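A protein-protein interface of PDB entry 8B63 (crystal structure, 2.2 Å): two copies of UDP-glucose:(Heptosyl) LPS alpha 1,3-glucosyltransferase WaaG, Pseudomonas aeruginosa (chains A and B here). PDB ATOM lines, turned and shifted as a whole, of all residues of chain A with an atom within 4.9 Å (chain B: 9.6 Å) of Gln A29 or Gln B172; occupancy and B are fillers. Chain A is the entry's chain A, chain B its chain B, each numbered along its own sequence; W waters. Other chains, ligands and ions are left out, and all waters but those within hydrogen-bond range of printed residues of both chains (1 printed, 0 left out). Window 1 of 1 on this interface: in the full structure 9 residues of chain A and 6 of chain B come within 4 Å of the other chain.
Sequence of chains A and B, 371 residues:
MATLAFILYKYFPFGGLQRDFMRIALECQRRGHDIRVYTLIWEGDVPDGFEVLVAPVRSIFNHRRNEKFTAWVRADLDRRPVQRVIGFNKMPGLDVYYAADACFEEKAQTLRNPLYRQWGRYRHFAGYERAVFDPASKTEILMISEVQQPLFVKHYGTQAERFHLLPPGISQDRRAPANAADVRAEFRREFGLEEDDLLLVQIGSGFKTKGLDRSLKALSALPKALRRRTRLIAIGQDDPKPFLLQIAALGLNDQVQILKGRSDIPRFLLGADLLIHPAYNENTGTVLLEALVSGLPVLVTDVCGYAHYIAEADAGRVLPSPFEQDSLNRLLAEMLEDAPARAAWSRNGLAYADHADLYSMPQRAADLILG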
ATOM      1  N   ALA A  25     -15.123 -20.999  26.644  1.00  0.00           N
ATOM      2  CA  ALA A  25     -14.627 -19.669  26.363  1.00  0.00           C
ATOM      3  C   ALA A  25     -13.138 -19.738  25.988  1.00  0.00           C
ATOM      4  O   ALA A  25     -12.718 -19.155  24.981  1.00  0.00           O
ATOM      5  CB  ALA A  25     -14.920 -18.781  27.562  1.00  0.00           C
ATOM      6  N   LEU A  26     -12.357 -20.494  26.761  1.00  0.00           N
ATOM      7  CA  LEU A  26     -10.958 -20.730  26.441  1.00  0.00           C
ATOM      8  C   LEU A  26     -10.808 -21.375  25.061  1.00  0.00           C
ATOM      9  O   LEU A  26      -9.879 -21.055  24.334  1.00  0.00           O
ATOM     10  CB  LEU A  26     -10.330 -21.606  27.529  1.00  0.00           C
ATOM     11  CG  LEU A  26     -10.054 -20.924  28.872  1.00  0.00           C
ATOM     12  CD1 LEU A  26      -9.581 -21.936  29.925  1.00  0.00           C
ATOM     13  CD2 LEU A  26      -9.007 -19.812  28.714  1.00  0.00           C
ATOM     14  N   GLU A  27     -11.725 -22.272  24.675  1.00  0.00           N
ATOM     15  CA  GLU A  27     -11.596 -22.953  23.388  1.00  0.00           C
ATOM     16  C   GLU A  27     -11.823 -21.934  22.263  1.00  0.00           C
ATOM     17  O   GLU A  27     -11.078 -21.916  21.280  1.00  0.00           O
ATOM     18  CB  GLU A  27     -12.548 -24.158  23.344  1.00  0.00           C
ATOM     19  CG  GLU A  27     -12.633 -24.892  22.001  1.00  0.00           C
ATOM     20  CD  GLU A  27     -11.348 -25.469  21.412  1.00  0.00           C
ATOM     21  OE1 GLU A  27     -10.424 -25.752  22.192  1.00  0.00           O
ATOM     22  OE2 GLU A  27     -11.273 -25.624  20.163  1.00  0.00           O
ATOM     23  N   CYS A  28     -12.878 -21.108  22.411  1.00  0.00           N
ATOM     24  CA  CYS A  28     -13.202 -20.085  21.428  1.00  0.00           C
ATOM     25  C   CYS A  28     -12.064 -19.061  21.341  1.00  0.00           C
ATOM     26  O   CYS A  28     -11.768 -18.591  20.251  1.00  0.00           O
ATOM     27  CB  CYS A  28     -14.522 -19.385  21.739  1.00  0.00           C
ATOM     28  SG  CYS A  28     -15.988 -20.455  21.661  1.00  0.00           S
ATOM     29  N   GLN A  29     -11.467 -18.713  22.493  1.00  0.00           N
ATOM     30  CA  GLN A  29     -10.332 -17.804  22.542  1.00  0.00           C
ATOM     31  C   GLN A  29      -9.167 -18.345  21.723  1.00  0.00           C
ATOM     32  O   GLN A  29      -8.461 -17.590  21.068  1.00  0.00           O
ATOM     33  CB  GLN A  29      -9.789 -17.620  23.966  1.00  0.00           C
ATOM     34  CG  GLN A  29      -8.694 -16.540  24.071  1.00  0.00           C
ATOM     35  CD  GLN A  29      -8.208 -16.346  25.490  1.00  0.00           C
ATOM     36  OE1 GLN A  29      -7.860 -17.312  26.175  1.00  0.00           O
ATOM     37  NE2 GLN A  29      -8.248 -15.106  25.964  1.00  0.00           N
ATOM     38  N   ARG A  30      -8.913 -19.644  21.865  1.00  0.00           N
ATOM     39  CA  ARG A  30      -7.757 -20.269  21.251  1.00  0.00           C
ATOM     40  C   ARG A  30      -7.942 -20.333  19.736  1.00  0.00           C
ATOM     41  O   ARG A  30      -6.971 -20.391  18.999  1.00  0.00           O
ATOM     42  CB  ARG A  30      -7.496 -21.614  21.937  1.00  0.00           C
ATOM     43  CG  ARG A  30      -6.889 -21.429  23.327  1.00  0.00           C
ATOM     44  CD  ARG A  30      -6.374 -22.695  24.006  1.00  0.00           C
ATOM     45  NE  ARG A  30      -7.431 -23.699  24.052  1.00  0.00           N
ATOM     46  CZ  ARG A  30      -7.804 -24.392  25.127  1.00  0.00           C
ATOM     47  NH1 ARG A  30      -8.979 -25.007  25.122  1.00  0.00           N
ATOM     48  NH2 ARG A  30      -7.031 -24.431  26.204  1.00  0.00           N
ATOM     49  N   ARG A  31      -9.190 -20.246  19.264  1.00  0.00           N
ATOM     50  CA  ARG A  31      -9.463 -20.197  17.834  1.00  0.00           C
ATOM     51  C   ARG A  31      -9.505 -18.758  17.295  1.00  0.00           C
ATOM     52  O   ARG A  31     -10.012 -18.560  16.197  1.00  0.00           O
ATOM     53  CB  ARG A  31     -10.778 -20.933  17.549  1.00  0.00           C
ATOM     54  CG  ARG A  31     -10.799 -22.383  18.021  1.00  0.00           C
ATOM     55  CD  ARG A  31     -12.078 -23.042  17.544  1.00  0.00           C
ATOM     56  NE  ARG A  31     -12.361 -24.372  18.080  1.00  0.00           N
ATOM     57  CZ  ARG A  31     -13.382 -25.128  17.689  1.00  0.00           C
ATOM     58  NH1 ARG A  31     -14.163 -24.715  16.711  1.00  0.00           N
ATOM     59  NH2 ARG A  31     -13.590 -26.326  18.209  1.00  0.00           N
ATOM     60  N   GLY A  32      -9.022 -17.765  18.060  1.00  0.00           N
ATOM     61  CA  GLY A  32      -8.812 -16.401  17.576  1.00  0.00           C
ATOM     62  C   GLY A  32      -9.901 -15.377  17.974  1.00  0.00           C
ATOM     63  O   GLY A  32     -10.054 -14.338  17.297  1.00  0.00           O
ATOM     64  N   HIS A  33     -10.639 -15.623  19.076  1.00  0.00           N
ATOM     65  CA  HIS A  33     -11.703 -14.705  19.499  1.00  0.00           C
ATOM     66  C   HIS A  33     -11.370 -14.081  20.854  1.00  0.00           C
ATOM     67  O   HIS A  33     -11.026 -14.794  21.802  1.00  0.00           O
ATOM     68  CB  HIS A  33     -13.082 -15.393  19.522  1.00  0.00           C
ATOM     69  CG  HIS A  33     -13.453 -15.979  18.210  1.00  0.00           C
ATOM     70  ND1 HIS A  33     -14.079 -15.232  17.234  1.00  0.00           N
ATOM     71  CD2 HIS A  33     -13.185 -17.163  17.641  1.00  0.00           C
ATOM     72  CE1 HIS A  33     -14.235 -15.984  16.144  1.00  0.00           C
ATOM     73  NE2 HIS A  33     -13.688 -17.152  16.354  1.00  0.00           N
ATOM     74  N   ILE A  35     -12.516 -12.332  24.340  1.00  0.00           N
ATOM     75  CA  ILE A  35     -13.566 -12.805  25.231  1.00  0.00           C
ATOM     76  C   ILE A  35     -14.005 -11.659  26.127  1.00  0.00           C
ATOM     77  O   ILE A  35     -13.215 -11.136  26.887  1.00  0.00           O
ATOM     78  CB  ILE A  35     -13.090 -13.998  26.090  1.00  0.00           C
ATOM     79  CG1 ILE A  35     -12.572 -15.166  25.243  1.00  0.00           C
ATOM     80  CG2 ILE A  35     -14.187 -14.415  27.060  1.00  0.00           C
ATOM     81  CD1 ILE A  35     -13.561 -15.686  24.251  1.00  0.00           C
ATOM     82  N   ASP A  48      -6.009 -14.608  31.087  1.00  0.00           N
ATOM     83  CA  ASP A  48      -5.431 -13.609  30.199  1.00  0.00           C
ATOM     84  C   ASP A  48      -6.385 -13.320  29.034  1.00  0.00           C
ATOM     85  O   ASP A  48      -6.894 -14.253  28.449  1.00  0.00           O
ATOM     86  CB  ASP A  48      -4.082 -14.082  29.638  1.00  0.00           C
ATOM     87  CG  ASP A  48      -2.997 -14.345  30.678  1.00  0.00           C
ATOM     88  OD1 ASP A  48      -3.262 -14.153  31.897  1.00  0.00           O
ATOM     89  OD2 ASP A  48      -1.886 -14.745  30.266  1.00  0.00           O
ATOM     90  N   GLY A  49      -6.637 -12.037  28.721  1.00  0.00           N
ATOM     91  CA  GLY A  49      -7.368 -11.643  27.523  1.00  0.00           C
ATOM     92  C   GLY A  49      -8.883 -11.574  27.726  1.00  0.00           C
ATOM     93  O   GLY A  49      -9.598 -11.171  26.808  1.00  0.00           O
ATOM     94  N   PHE A  50      -9.361 -11.940  28.933  1.00  0.00           N
ATOM     95  CA  PHE A  50     -10.785 -11.935  29.240  1.00  0.00           C
ATOM     96  C   PHE A  50     -11.183 -10.565  29.796  1.00  0.00           C
ATOM     97  O   PHE A  50     -10.701 -10.193  30.864  1.00  0.00           O
ATOM     98  CB  PHE A  50     -11.143 -13.016  30.270  1.00  0.00           C
ATOM     99  CG  PHE A  50     -11.391 -14.408  29.748  1.00  0.00           C
ATOM    100  CD1 PHE A  50     -10.543 -14.997  28.822  1.00  0.00           C
ATOM    101  CD2 PHE A  50     -12.436 -15.174  30.258  1.00  0.00           C
ATOM    102  CE1 PHE A  50     -10.784 -16.291  28.365  1.00  0.00           C
ATOM    103  CE2 PHE A  50     -12.670 -16.461  29.801  1.00  0.00           C
ATOM    104  CZ  PHE A  50     -11.843 -17.013  28.850  1.00  0.00           C
ATOM    105  N   ARG B  19       8.883  -8.569  29.677  1.00  0.00           N
ATOM    106  CA  ARG B  19       7.602  -9.269  29.480  1.00  0.00           C
ATOM    107  C   ARG B  19       7.678 -10.718  29.963  1.00  0.00           C
ATOM    108  O   ARG B  19       6.685 -11.285  30.432  1.00  0.00           O
ATOM    109  CB  ARG B  19       7.164  -9.223  28.008  1.00  0.00           C
ATOM    110  CG  ARG B  19       6.741  -7.835  27.530  1.00  0.00           C
ATOM    111  CD  ARG B  19       6.506  -7.690  26.034  1.00  0.00           C
ATOM    112  NE  ARG B  19       5.661  -8.742  25.449  1.00  0.00           N
ATOM    113  CZ  ARG B  19       4.326  -8.786  25.476  1.00  0.00           C
ATOM    114  NH1 ARG B  19       3.622  -7.746  25.867  1.00  0.00           N
ATOM    115  NH2 ARG B  19       3.695  -9.844  25.010  1.00  0.00           N
ATOM    116  N   ARG B  23       5.386 -12.166  33.054  1.00  0.00           N
ATOM    117  CA  ARG B  23       4.500 -13.288  32.810  1.00  0.00           C
ATOM    118  C   ARG B  23       4.813 -14.432  33.778  1.00  0.00           C
ATOM    119  O   ARG B  23       3.925 -15.158  34.212  1.00  0.00           O
ATOM    120  CB  ARG B  23       4.613 -13.698  31.339  1.00  0.00           C
ATOM    121  CG  ARG B  23       3.855 -12.795  30.364  1.00  0.00           C
ATOM    122  CD  ARG B  23       3.628 -13.489  29.021  1.00  0.00           C
ATOM    123  NE  ARG B  23       2.614 -14.555  29.032  1.00  0.00           N
ATOM    124  CZ  ARG B  23       2.552 -15.607  28.200  1.00  0.00           C
ATOM    125  NH1 ARG B  23       1.698 -16.594  28.431  1.00  0.00           N
ATOM    126  NH2 ARG B  23       3.397 -15.731  27.191  1.00  0.00           N
ATOM    127  N   PRO B 168       9.257 -21.489  24.111  1.00  0.00           N
ATOM    128  CA  PRO B 168       8.845 -20.078  24.090  1.00  0.00           C
ATOM    129  C   PRO B 168       7.583 -19.686  24.871  1.00  0.00           C
ATOM    130  O   PRO B 168       6.751 -20.537  25.204  1.00  0.00           O
ATOM    131  CB  PRO B 168       8.641 -19.805  22.580  1.00  0.00           C
ATOM    132  CG  PRO B 168       9.420 -20.923  21.872  1.00  0.00           C
ATOM    133  CD  PRO B 168       9.257 -22.121  22.781  1.00  0.00           C
ATOM    134  N   GLY B 169       7.449 -18.372  25.136  1.00  0.00           N
ATOM    135  CA  GLY B 169       6.348 -17.807  25.902  1.00  0.00           C
ATOM    136  C   GLY B 169       5.658 -16.631  25.203  1.00  0.00           C
ATOM    137  O   GLY B 169       5.398 -15.609  25.839  1.00  0.00           O
ATOM    138  N   ILE B 170       5.374 -16.788  23.900  1.00  0.00           N
ATOM    139  CA  ILE B 170       4.622 -15.814  23.122  1.00  0.00           C
ATOM    140  C   ILE B 170       3.269 -15.593  23.778  1.00  0.00           C
ATOM    141  O   ILE B 170       2.581 -16.572  24.085  1.00  0.00           O
ATOM    142  CB  ILE B 170       4.414 -16.329  21.685  1.00  0.00           C
ATOM    143  CG1 ILE B 170       5.734 -16.621  20.946  1.00  0.00           C
ATOM    144  CG2 ILE B 170       3.478 -15.390  20.917  1.00  0.00           C
ATOM    145  CD1 ILE B 170       6.907 -15.715  21.309  1.00  0.00           C
ATOM    146  N   SER B 171       2.844 -14.347  23.945  1.00  0.00           N
ATOM    147  CA  SER B 171       1.524 -14.199  24.529  1.00  0.00           C
ATOM    148  C   SER B 171       0.456 -14.424  23.438  1.00  0.00           C
ATOM    149  O   SER B 171       0.703 -14.243  22.234  1.00  0.00           O
ATOM    150  CB  SER B 171       1.379 -12.911  25.375  1.00  0.00           C
ATOM    151  OG  SER B 171       1.552 -11.717  24.629  1.00  0.00           O
ATOM    152  N   GLN B 172      -0.706 -14.911  23.893  1.00  0.00           N
ATOM    153  CA  GLN B 172      -1.860 -15.290  23.079  1.00  0.00           C
ATOM    154  C   GLN B 172      -2.380 -14.161  22.190  1.00  0.00           C
ATOM    155  O   GLN B 172      -3.016 -14.422  21.164  1.00  0.00           O
ATOM    156  CB  GLN B 172      -3.059 -15.653  23.962  1.00  0.00           C
ATOM    157  CG  GLN B 172      -3.094 -17.089  24.463  1.00  0.00           C
ATOM    158  CD  GLN B 172      -4.486 -17.497  24.904  1.00  0.00           C
ATOM    159  OE1 GLN B 172      -5.481 -16.891  24.506  1.00  0.00           O
ATOM    160  NE2 GLN B 172      -4.571 -18.550  25.710  1.00  0.00           N
ATOM    161  N   ASP B 173      -2.228 -12.909  22.650  1.00  0.00           N
ATOM    162  CA  ASP B 173      -2.764 -11.755  21.934  1.00  0.00           C
ATOM    163  C   ASP B 173      -2.026 -11.607  20.593  1.00  0.00           C
ATOM    164  O   ASP B 173      -2.516 -10.932  19.682  1.00  0.00           O
ATOM    165  CB  ASP B 173      -2.797 -10.489  22.817  1.00  0.00           C
ATOM    166  CG  ASP B 173      -1.469 -10.024  23.422  1.00  0.00           C
ATOM    167  OD1 ASP B 173      -0.588 -10.850  23.675  1.00  0.00           O
ATOM    168  OD2 ASP B 173      -1.319  -8.832  23.643  1.00  0.00           O
ATOM    169  N   ARG B 174      -0.839 -12.235  20.450  1.00  0.00           N
ATOM    170  CA  ARG B 174      -0.063 -12.056  19.224  1.00  0.00           C
ATOM    171  C   ARG B 174      -0.581 -12.974  18.129  1.00  0.00           C
ATOM    172  O   ARG B 174      -0.226 -12.792  16.971  1.00  0.00           O
ATOM    173  CB  ARG B 174       1.438 -12.299  19.419  1.00  0.00           C
ATOM    174  CG  ARG B 174       2.227 -11.031  19.700  1.00  0.00           C
ATOM    175  CD  ARG B 174       2.066 -10.559  21.129  1.00  0.00           C
ATOM    176  NE  ARG B 174       2.984  -9.472  21.425  1.00  0.00           N
ATOM    177  CZ  ARG B 174       2.683  -8.374  22.094  1.00  0.00           C
ATOM    178  NH1 ARG B 174       1.434  -8.159  22.465  1.00  0.00           N
ATOM    179  NH2 ARG B 174       3.640  -7.489  22.344  1.00  0.00           N
ATOM    180  N   ARG B 175      -1.404 -13.956  18.508  1.00  0.00           N
ATOM    181  CA  ARG B 175      -1.898 -14.926  17.547  1.00  0.00           C
ATOM    182  C   ARG B 175      -2.941 -14.265  16.657  1.00  0.00           C
ATOM    183  O   ARG B 175      -3.776 -13.520  17.158  1.00  0.00           O
ATOM    184  CB  ARG B 175      -2.459 -16.136  18.289  1.00  0.00           C
ATOM    185  CG  ARG B 175      -1.432 -16.815  19.187  1.00  0.00           C
ATOM    186  CD  ARG B 175      -1.985 -18.114  19.710  1.00  0.00           C
ATOM    187  NE  ARG B 175      -2.157 -19.009  18.583  1.00  0.00           N
ATOM    188  CZ  ARG B 175      -3.065 -19.967  18.515  1.00  0.00           C
ATOM    189  NH1 ARG B 175      -3.968 -20.092  19.474  1.00  0.00           N
ATOM    190  NH2 ARG B 175      -3.078 -20.757  17.456  1.00  0.00           N
ATOM    191  N   ALA B 176      -2.863 -14.519  15.342  1.00  0.00           N
ATOM    192  CA  ALA B 176      -3.854 -13.991  14.411  1.00  0.00           C
ATOM    193  C   ALA B 176      -5.251 -14.283  14.955  1.00  0.00           C
ATOM    194  O   ALA B 176      -5.566 -15.431  15.298  1.00  0.00           O
ATOM    195  CB  ALA B 176      -3.688 -14.571  13.021  1.00  0.00           C
ATOM    196  N   PRO B 177      -6.104 -13.242  15.094  1.00  0.00           N
ATOM    197  CA  PRO B 177      -7.515 -13.447  15.450  1.00  0.00           C
ATOM    198  C   PRO B 177      -8.363 -13.856  14.239  1.00  0.00           C
ATOM    199  O   PRO B 177      -7.915 -13.752  13.094  1.00  0.00           O
ATOM    200  CB  PRO B 177      -7.856 -12.067  16.056  1.00  0.00           C
ATOM    201  CG  PRO B 177      -7.071 -11.092  15.189  1.00  0.00           C
ATOM    202  CD  PRO B 177      -5.753 -11.812  14.973  1.00  0.00           C
ATOM    203  N   ALA B 178      -9.581 -14.343  14.504  1.00  0.00           N
ATOM    204  CA  ALA B 178     -10.529 -14.729  13.459  1.00  0.00           C
ATOM    205  C   ALA B 178     -10.858 -13.562  12.515  1.00  0.00           C
ATOM    206  O   ALA B 178     -11.278 -13.778  11.401  1.00  0.00           O
ATOM    207  CB  ALA B 178     -11.818 -15.265  14.086  1.00  0.00           C
ATOM    208  N   PRO B 266       0.519  -6.300  17.866  1.00  0.00           N
ATOM    209  CA  PRO B 266      -0.212  -7.247  17.026  1.00  0.00           C
ATOM    210  C   PRO B 266      -0.909  -6.640  15.806  1.00  0.00           C
ATOM    211  O   PRO B 266      -1.080  -7.337  14.805  1.00  0.00           O
ATOM    212  CB  PRO B 266      -1.235  -7.875  17.982  1.00  0.00           C
ATOM    213  CG  PRO B 266      -0.582  -7.746  19.340  1.00  0.00           C
ATOM    214  CD  PRO B 266       0.142  -6.422  19.275  1.00  0.00           C
ATOM    215  N   LEU B 270      -0.164  -7.659  11.882  1.00  0.00           N
ATOM    216  CA  LEU B 270      -1.204  -8.011  10.913  1.00  0.00           C
ATOM    217  C   LEU B 270      -1.227  -7.070   9.697  1.00  0.00           C
ATOM    218  O   LEU B 270      -1.612  -7.469   8.586  1.00  0.00           O
ATOM    219  CB  LEU B 270      -2.539  -8.003  11.664  1.00  0.00           C
ATOM    220  CG  LEU B 270      -2.730  -9.137  12.687  1.00  0.00           C
ATOM    221  CD1 LEU B 270      -3.858  -8.839  13.643  1.00  0.00           C
ATOM    222  CD2 LEU B 270      -3.009 -10.474  12.003  1.00  0.00           C
ATOM    223  N   GLU B 290       6.529 -13.889  17.121  1.00  0.00           N
ATOM    224  CA  GLU B 290       5.299 -13.107  17.150  1.00  0.00           C
ATOM    225  C   GLU B 290       4.808 -12.827  15.716  1.00  0.00           C
ATOM    226  O   GLU B 290       3.622 -12.927  15.418  1.00  0.00           O
ATOM    227  CB  GLU B 290       5.529 -11.808  17.926  1.00  0.00           C
ATOM    228  CG  GLU B 290       5.657 -11.977  19.432  1.00  0.00           C
ATOM    229  CD  GLU B 290       5.885 -10.675  20.202  1.00  0.00           C
ATOM    230  OE1 GLU B 290       6.389  -9.714  19.566  1.00  0.00           O
ATOM    231  OE2 GLU B 290       5.554 -10.599  21.430  1.00  0.00           O
ATOM    232  N   VAL B 293       3.272 -16.283  14.456  1.00  0.00           N
ATOM    233  CA  VAL B 293       1.911 -16.617  14.861  1.00  0.00           C
ATOM    234  C   VAL B 293       0.921 -15.571  14.328  1.00  0.00           C
ATOM    235  O   VAL B 293      -0.267 -15.825  14.345  1.00  0.00           O
ATOM    236  CB  VAL B 293       1.782 -16.795  16.380  1.00  0.00           C
ATOM    237  CG1 VAL B 293       2.753 -17.842  16.914  1.00  0.00           C
ATOM    238  CG2 VAL B 293       1.963 -15.480  17.106  1.00  0.00           C
ATOM    239  N   SER B 294       1.388 -14.419  13.826  1.00  0.00           N
ATOM    240  CA  SER B 294       0.513 -13.479  13.156  1.00  0.00           C
ATOM    241  C   SER B 294       0.398 -13.782  11.654  1.00  0.00           C
ATOM    242  O   SER B 294      -0.430 -13.198  10.957  1.00  0.00           O
ATOM    243  CB  SER B 294       0.932 -12.054  13.395  1.00  0.00           C
ATOM    244  OG  SER B 294       0.987 -11.768  14.776  1.00  0.00           O
ATOM    245  N   ALA B 353       2.028 -22.322  14.044  1.00  0.00           N
ATOM    246  CA  ALA B 353       1.480 -21.742  15.272  1.00  0.00           C
ATOM    247  C   ALA B 353       0.418 -22.644  15.908  1.00  0.00           C
ATOM    248  O   ALA B 353       0.241 -22.600  17.123  1.00  0.00           O
ATOM    249  CB  ALA B 353       0.908 -20.359  15.018  1.00  0.00           C
ATOM    250  N   ASP B 354      -0.259 -23.468  15.097  1.00  0.00           N
ATOM    251  CA  ASP B 354      -1.338 -24.334  15.553  1.00  0.00           C
ATOM    252  C   ASP B 354      -0.769 -25.656  16.075  1.00  0.00           C
ATOM    253  O   ASP B 354      -1.437 -26.384  16.792  1.00  0.00           O
ATOM    254  CB  ASP B 354      -2.349 -24.476  14.406  1.00  0.00           C
ATOM    255  CG  ASP B 354      -3.786 -24.181  14.802  1.00  0.00           C
ATOM    256  OD1 ASP B 354      -3.981 -23.304  15.663  1.00  0.00           O
ATOM    257  OD2 ASP B 354      -4.703 -24.804  14.224  1.00  0.00           O
ATOM    258  N   LEU B 358       4.659 -22.855  21.718  1.00  0.00           N
ATOM    259  CA  LEU B 358       5.372 -21.593  21.621  1.00  0.00           C
ATOM    260  C   LEU B 358       4.906 -20.648  22.723  1.00  0.00           C
ATOM    261  O   LEU B 358       5.301 -19.489  22.702  1.00  0.00           O
ATOM    262  CB  LEU B 358       5.095 -20.958  20.250  1.00  0.00           C
ATOM    263  CG  LEU B 358       5.577 -21.696  19.000  1.00  0.00           C
ATOM    264  CD1 LEU B 358       5.378 -20.824  17.754  1.00  0.00           C
ATOM    265  CD2 LEU B 358       7.023 -22.123  19.123  1.00  0.00           C
ATOM    266  N   TYR B 359       4.096 -21.152  23.668  1.00  0.00           N
ATOM    267  CA  TYR B 359       3.259 -20.331  24.545  1.00  0.00           C
ATOM    268  C   TYR B 359       3.562 -20.567  26.027  1.00  0.00           C
ATOM    269  O   TYR B 359       3.390 -19.667  26.857  1.00  0.00           O
ATOM    270  CB  TYR B 359       1.770 -20.592  24.234  1.00  0.00           C
ATOM    271  CG  TYR B 359       1.466 -20.571  22.758  1.00  0.00           C
ATOM    272  CD1 TYR B 359       1.582 -19.383  22.052  1.00  0.00           C
ATOM    273  CD2 TYR B 359       1.168 -21.722  22.034  1.00  0.00           C
ATOM    274  CE1 TYR B 359       1.383 -19.326  20.683  1.00  0.00           C
ATOM    275  CE2 TYR B 359       0.949 -21.678  20.662  1.00  0.00           C
ATOM    276  CZ  TYR B 359       1.057 -20.471  19.984  1.00  0.00           C
ATOM    277  OH  TYR B 359       0.887 -20.291  18.632  1.00  0.00           O
ATOM    278  N   SER B 360       4.023 -21.777  26.362  1.00  0.00           N
ATOM    279  CA  SER B 360       3.840 -22.314  27.704  1.00  0.00           C
ATOM    280  C   SER B 360       5.001 -21.995  28.651  1.00  0.00           C
ATOM    281  O   SER B 360       4.997 -22.496  29.789  1.00  0.00           O
ATOM    282  CB  SER B 360       3.592 -23.819  27.635  1.00  0.00           C
ATOM    283  OG  SER B 360       4.739 -24.545  27.195  1.00  0.00           O
ATOM    284  N   PRO B 362       5.835 -19.602  30.650  1.00  0.00           N
ATOM    285  CA  PRO B 362       5.628 -19.096  32.011  1.00  0.00           C
ATOM    286  C   PRO B 362       5.238 -20.200  33.007  1.00  0.00           C
ATOM    287  O   PRO B 362       5.754 -20.247  34.124  1.00  0.00           O
ATOM    288  CB  PRO B 362       4.540 -18.028  31.841  1.00  0.00           C
ATOM    289  CG  PRO B 362       4.480 -17.732  30.337  1.00  0.00           C
ATOM    290  CD  PRO B 362       4.903 -19.012  29.663  1.00  0.00           C
ATOM    291  N   GLN B 363       4.348 -21.105  32.602  1.00  0.00           N
ATOM    292  CA  GLN B 363       3.933 -22.196  33.481  1.00  0.00           C
ATOM    293  C   GLN B 363       5.130 -23.101  33.770  1.00  0.00           C
ATOM    294  O   GLN B 363       5.271 -23.574  34.897  1.00  0.00           O
ATOM    295  CB  GLN B 363       2.795 -23.040  32.898  1.00  0.00           C
ATOM    296  CG  GLN B 363       1.473 -22.293  32.752  1.00  0.00           C
ATOM    297  CD  GLN B 363       1.512 -21.242  31.670  1.00  0.00           C
ATOM    298  OE1 GLN B 363       1.605 -21.543  30.477  1.00  0.00           O
ATOM    299  NE2 GLN B 363       1.445 -19.984  32.085  1.00  0.00           N
HETATM  300  O   HOH W   1      -7.303 -19.668  25.680  1.00  0.00           O
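Gln A29 touches just one residue of chain B: Gln B172 (2.9 Å). Of the printed residues of chain A, Gln B172 touches Gln A29. No residue of chain B comes within 4 Å of Cys A28. Of chain B, only Pro B177 and Ala B178 come within 4 Å of Gly A32. No residue of chain B comes within 4 Å of Gly A49. Printed residues of chain B within 4 Å of His A33: Ala B178. Printed residues of chain A within 4 Å of Arg B175: Arg A30. Ile A35 touches none of the printed residues of chain B. The nearest residue of chain B that does not touch Gln A29 is Arg B175 (5.4 Å). The nearest printed residue of chain A that does not touch Ala B178 is Arg A31 (4.3 Å).
Water W1 lies within hydrogen-bond range of OE1 of Gln A29 (2.5 Å), NE2 of Gln B172 (3.0 Å) and O of Leu A26 (3.2 Å).
Printed residues of chain A that touch a printed residue of chain B: Gln A29, Arg A30, Gly A32 and His A33. Hydrophobic or aromatic side chains of chain B within 4 Å of the printed part of chain A: Pro B177 and Ala B178. Among the printed residues, 5 pairs touch across the chains.
Among the printed residues, merely in contact across the chains: Gly A32 with Pro B177 (3.3 Å) and His A33 with Ala B178 (3.3 Å).
O of Gly A32 lies within hydrogen-bond range of N of Ala B178 (2.8 Å). The side-chain amide oxygen (OE1) of Gln B172 sits close to the side-chain amide oxygen (OE1) of Gln A29. O of Arg A30 sits at hydrogen-bond distance from NH1 of Arg B175, 3.1 Å away.
No position is printed for both chains. Of the 5 pairs that touch across the chains among the printed residues, none has its exchanged pair printed and touching as well.
The backbone carbonyl oxygen (O) of Cys A28 lies close to the backbone NH (N) of His A33 (3.4 Å). The side-chain carboxylate of Glu A27 is in salt-bridge range of the guanidinium group of Arg A30. The side-chain amide nitrogen (NE2) of Gln A29 sits at hydrogen-bond distance from the backbone carbonyl oxygen (O) of Asp A48 (3.0 Å). The guanidinium group of Arg B175 lies within salt-bridge range of the side-chain carboxylate of Asp B354 (3.2 Å). The guanidinium group (NE) of Arg B175 is in hydrogen-bond range of the side-chain hydroxyl (OH) of Tyr B359 (3.3 Å).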
